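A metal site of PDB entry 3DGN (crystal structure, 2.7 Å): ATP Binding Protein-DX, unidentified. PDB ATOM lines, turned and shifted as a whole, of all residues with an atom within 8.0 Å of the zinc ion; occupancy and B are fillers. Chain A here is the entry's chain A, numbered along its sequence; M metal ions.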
ATOM      1  N   PRO A  24       0.640  19.560   3.554  1.00  0.00           N
ATOM      2  CA  PRO A  24       0.495  20.995   3.812  1.00  0.00           C
ATOM      3  C   PRO A  24       1.737  21.537   4.513  1.00  0.00           C
ATOM      4  O   PRO A  24       2.531  20.717   4.998  1.00  0.00           O
ATOM      5  CB  PRO A  24      -0.744  21.097   4.746  1.00  0.00           C
ATOM      6  CG  PRO A  24      -0.934  19.698   5.346  1.00  0.00           C
ATOM      7  CD  PRO A  24       0.008  18.725   4.611  1.00  0.00           C
ATOM      8  N   CYS A  25       1.916  22.875   4.543  1.00  0.00           N
ATOM      9  CA  CYS A  25       2.981  23.553   5.335  1.00  0.00           C
ATOM     10  C   CYS A  25       3.549  22.736   6.554  1.00  0.00           C
ATOM     11  O   CYS A  25       2.759  22.429   7.441  1.00  0.00           O
ATOM     12  CB  CYS A  25       2.418  24.844   5.898  1.00  0.00           C
ATOM     13  SG  CYS A  25       3.726  25.745   6.804  1.00  0.00           S
ATOM     14  N   VAL A  26       4.842  22.384   6.648  1.00  0.00           N
ATOM     15  CA  VAL A  26       5.301  21.765   7.914  1.00  0.00           C
ATOM     16  C   VAL A  26       4.883  22.523   9.251  1.00  0.00           C
ATOM     17  O   VAL A  26       4.679  21.866  10.311  1.00  0.00           O
ATOM     18  CB  VAL A  26       6.770  21.518   7.968  1.00  0.00           C
ATOM     19  CG1 VAL A  26       7.220  20.420   6.916  1.00  0.00           C
ATOM     20  CG2 VAL A  26       7.554  22.869   7.876  1.00  0.00           C
ATOM     21  N   LYS A  27       4.737  23.853   9.209  1.00  0.00           N
ATOM     22  CA  LYS A  27       4.638  24.633  10.445  1.00  0.00           C
ATOM     23  C   LYS A  27       3.191  24.794  10.907  1.00  0.00           C
ATOM     24  O   LYS A  27       2.828  24.282  11.941  1.00  0.00           O
ATOM     25  CB  LYS A  27       5.380  26.003  10.355  1.00  0.00           C
ATOM     26  CG  LYS A  27       5.299  26.792  11.662  1.00  0.00           C
ATOM     27  CD  LYS A  27       5.996  26.139  12.785  1.00  0.00           C
ATOM     28  CE  LYS A  27       5.990  26.997  14.020  1.00  0.00           C
ATOM     29  NZ  LYS A  27       6.619  26.333  15.289  1.00  0.00           N
ATOM     30  N   CYS A  28       2.367  25.549  10.162  1.00  0.00           N
ATOM     31  CA  CYS A  28       0.934  25.641  10.420  1.00  0.00           C
ATOM     32  C   CYS A  28       0.137  24.362  10.119  1.00  0.00           C
ATOM     33  O   CYS A  28      -0.884  24.112  10.688  1.00  0.00           O
ATOM     34  CB  CYS A  28       0.360  26.832   9.659  1.00  0.00           C
ATOM     35  SG  CYS A  28       0.074  26.467   7.892  1.00  0.00           S
ATOM     36  N   LYS A  29       0.608  23.562   9.219  1.00  0.00           N
ATOM     37  CA  LYS A  29      -0.004  22.268   8.783  1.00  0.00           C
ATOM     38  C   LYS A  29      -1.409  22.302   8.195  1.00  0.00           C
ATOM     39  O   LYS A  29      -2.073  21.293   8.131  1.00  0.00           O
ATOM     40  CB  LYS A  29       0.264  21.049   9.706  1.00  0.00           C
ATOM     41  CG  LYS A  29      -0.022  21.206  11.161  1.00  0.00           C
ATOM     42  CD  LYS A  29       1.260  21.176  12.093  1.00  0.00           C
ATOM     43  CE  LYS A  29       1.892  19.807  12.438  1.00  0.00           C
ATOM     44  NZ  LYS A  29       2.935  19.543  11.395  1.00  0.00           N
ATOM     45  N   VAL A  30      -1.792  23.483   7.705  1.00  0.00           N
ATOM     46  CA  VAL A  30      -3.071  23.704   7.033  1.00  0.00           C
ATOM     47  C   VAL A  30      -2.740  24.421   5.742  1.00  0.00           C
ATOM     48  O   VAL A  30      -3.105  23.947   4.705  1.00  0.00           O
ATOM     49  CB  VAL A  30      -4.032  24.569   7.900  1.00  0.00           C
ATOM     50  CG1 VAL A  30      -5.312  24.996   7.128  1.00  0.00           C
ATOM     51  CG2 VAL A  30      -4.319  23.848   9.224  1.00  0.00           C
ATOM     52  N   ALA A  31      -1.988  25.542   5.760  1.00  0.00           N
ATOM     53  CA  ALA A  31      -1.798  26.221   4.449  1.00  0.00           C
ATOM     54  C   ALA A  31      -0.974  25.340   3.561  1.00  0.00           C
ATOM     55  O   ALA A  31      -0.174  24.506   4.054  1.00  0.00           O
ATOM     56  CB  ALA A  31      -1.160  27.547   4.576  1.00  0.00           C
ATOM     57  N   PRO A  32      -1.146  25.469   2.245  1.00  0.00           N
ATOM     58  CA  PRO A  32      -0.188  24.560   1.557  1.00  0.00           C
ATOM     59  C   PRO A  32       1.157  25.256   1.301  1.00  0.00           C
ATOM     60  O   PRO A  32       1.355  26.388   1.678  1.00  0.00           O
ATOM     61  CB  PRO A  32      -0.959  24.159   0.272  1.00  0.00           C
ATOM     62  CG  PRO A  32      -1.911  25.343   0.046  1.00  0.00           C
ATOM     63  CD  PRO A  32      -2.334  25.782   1.433  1.00  0.00           C
ATOM     64  N   ARG A  33       2.084  24.565   0.659  1.00  0.00           N
ATOM     65  CA  ARG A  33       3.469  25.064   0.608  1.00  0.00           C
ATOM     66  C   ARG A  33       3.778  26.083  -0.482  1.00  0.00           C
ATOM     67  O   ARG A  33       3.226  26.044  -1.597  1.00  0.00           O
ATOM     68  CB  ARG A  33       4.477  23.893   0.531  1.00  0.00           C
ATOM     69  CG  ARG A  33       4.291  22.925   1.639  1.00  0.00           C
ATOM     70  CD  ARG A  33       5.344  21.940   1.821  1.00  0.00           C
ATOM     71  NE  ARG A  33       4.942  20.951   2.802  1.00  0.00           N
ATOM     72  CZ  ARG A  33       5.687  19.859   3.093  1.00  0.00           C
ATOM     73  NH1 ARG A  33       6.854  19.666   2.439  1.00  0.00           N
ATOM     74  NH2 ARG A  33       5.328  18.972   4.021  1.00  0.00           N
ATOM     75  N   ASP A  34       4.727  26.976  -0.166  1.00  0.00           N
ATOM     76  CA  ASP A  34       5.279  27.897  -1.166  1.00  0.00           C
ATOM     77  C   ASP A  34       6.091  27.029  -2.047  1.00  0.00           C
ATOM     78  O   ASP A  34       6.546  25.988  -1.572  1.00  0.00           O
ATOM     79  CB  ASP A  34       6.217  28.908  -0.461  1.00  0.00           C
ATOM     80  CG  ASP A  34       6.603  30.123  -1.359  1.00  0.00           C
ATOM     81  OD1 ASP A  34       5.979  30.333  -2.428  1.00  0.00           O
ATOM     82  OD2 ASP A  34       7.547  30.873  -0.988  1.00  0.00           O
ATOM     83  N   ASN A  46       9.472  23.702   2.365  1.00  0.00           N
ATOM     84  CA  ASN A  46       8.697  23.133   3.476  1.00  0.00           C
ATOM     85  C   ASN A  46       7.473  23.967   4.071  1.00  0.00           C
ATOM     86  O   ASN A  46       6.485  23.408   4.550  1.00  0.00           O
ATOM     87  CB  ASN A  46       9.665  22.768   4.588  1.00  0.00           C
ATOM     88  CG  ASN A  46      10.770  21.953   4.100  1.00  0.00           C
ATOM     89  OD1 ASN A  46      10.633  21.255   3.085  1.00  0.00           O
ATOM     90  ND2 ASN A  46      11.878  21.983   4.807  1.00  0.00           N
ATOM     91  N   MET A  47       7.571  25.300   4.021  1.00  0.00           N
ATOM     92  CA  MET A  47       6.570  26.171   4.619  1.00  0.00           C
ATOM     93  C   MET A  47       5.678  26.979   3.657  1.00  0.00           C
ATOM     94  O   MET A  47       6.019  27.200   2.459  1.00  0.00           O
ATOM     95  CB  MET A  47       7.297  27.123   5.571  1.00  0.00           C
ATOM     96  CG  MET A  47       7.721  26.401   6.850  1.00  0.00           C
ATOM     97  SD  MET A  47       8.269  27.488   8.163  1.00  0.00           S
ATOM     98  CE  MET A  47       9.932  27.974   7.628  1.00  0.00           C
ATOM     99  N   CYS A  48       4.504  27.413   4.165  1.00  0.00           N
ATOM    100  CA  CYS A  48       3.735  28.315   3.335  1.00  0.00           C
ATOM    101  C   CYS A  48       4.435  29.723   3.397  1.00  0.00           C
ATOM    102  O   CYS A  48       5.365  29.960   4.148  1.00  0.00           O
ATOM    103  CB  CYS A  48       2.295  28.348   3.821  1.00  0.00           C
ATOM    104  SG  CYS A  48       2.145  29.130   5.451  1.00  0.00           S
ATOM    105  N   LYS A  49       4.042  30.685   2.606  1.00  0.00           N
ATOM    106  CA  LYS A  49       4.756  31.896   2.667  1.00  0.00           C
ATOM    107  C   LYS A  49       4.684  32.515   4.080  1.00  0.00           C
ATOM    108  O   LYS A  49       5.733  32.903   4.636  1.00  0.00           O
ATOM    109  CB  LYS A  49       4.180  32.861   1.659  1.00  0.00           C
ATOM    110  CG  LYS A  49       5.121  34.019   1.351  1.00  0.00           C
ATOM    111  CD  LYS A  49       6.402  33.550   0.661  1.00  0.00           C
ATOM    112  CE  LYS A  49       7.483  34.530   0.918  1.00  0.00           C
ATOM    113  NZ  LYS A  49       8.632  34.110   0.073  1.00  0.00           N
ATOM    114  N   THR A  50       3.477  32.621   4.657  1.00  0.00           N
ATOM    115  CA  THR A  50       3.259  33.365   5.885  1.00  0.00           C
ATOM    116  C   THR A  50       4.186  32.778   6.971  1.00  0.00           C
ATOM    117  O   THR A  50       4.959  33.537   7.621  1.00  0.00           O
ATOM    118  CB  THR A  50       1.858  33.160   6.461  1.00  0.00           C
ATOM    119  OG1 THR A  50       0.823  33.214   5.436  1.00  0.00           O
ATOM    120  CG2 THR A  50       1.631  34.166   7.556  1.00  0.00           C
ATOM    121  N   CYS A  51       4.136  31.441   7.167  1.00  0.00           N
ATOM    122  CA  CYS A  51       4.936  30.853   8.248  1.00  0.00           C
ATOM    123  C   CYS A  51       6.388  31.039   7.957  1.00  0.00           C
ATOM    124  O   CYS A  51       7.160  31.286   8.873  1.00  0.00           O
ATOM    125  CB  CYS A  51       4.671  29.359   8.427  1.00  0.00           C
ATOM    126  SG  CYS A  51       3.031  29.046   8.966  1.00  0.00           S
ATOM    127  N   PHE A  52       6.793  30.889   6.699  1.00  0.00           N
ATOM    128  CA  PHE A  52       8.198  31.129   6.365  1.00  0.00           C
ATOM    129  C   PHE A  52       8.762  32.519   6.814  1.00  0.00           C
ATOM    130  O   PHE A  52       9.838  32.596   7.540  1.00  0.00           O
ATOM    131  CB  PHE A  52       8.511  30.945   4.895  1.00  0.00           C
ATOM    132  CG  PHE A  52       9.909  31.248   4.598  1.00  0.00           C
ATOM    133  CD1 PHE A  52      10.914  30.520   5.209  1.00  0.00           C
ATOM    134  CD2 PHE A  52      10.244  32.338   3.723  1.00  0.00           C
ATOM    135  CE1 PHE A  52      12.327  30.838   4.937  1.00  0.00           C
ATOM    136  CE2 PHE A  52      11.576  32.694   3.406  1.00  0.00           C
ATOM    137  CZ  PHE A  52      12.673  31.950   4.043  1.00  0.00           C
HETATM  138 ZN    ZN M   1       2.274  27.499   7.351  1.00  0.00          ZN
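The backbone carbonyl oxygen (O) of Ala 31 lies within hydrogen-bond range of the backbone NH (N) of Cys 25, 2.7 Å away.
The side-chain sulfur of Cys 25 lies close to the backbone NH of Lys 27.
The backbone NH (N) of Ala 31 sits close to the side-chain sulfur (SG) of Cys 28, 3.1 Å away.
The side-chain sulfur (SG) of Cys 28 sits close to the backbone NH (N) of Val 30 (3.5 Å).
Within 4 Å of the zinc ion: Cys 25, Cys 28, Cys 48 and Cys 51.
The nearest printed residue that does not touch the zinc ion is Ala 31 (4.4 Å).
The side-chain sulfur (SG) of Cys 25 binds the zinc ion (2.3 Å).
The side-chain sulfur (SG) of Cys 51 binds the zinc ion (2.4 Å).
SG of Cys 28 is bound to the zinc ion (2.5 Å).
SG of Cys 48 is bound to the zinc ion, at 2.5 Å.
The zinc ion has four donor atoms within binding distance.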
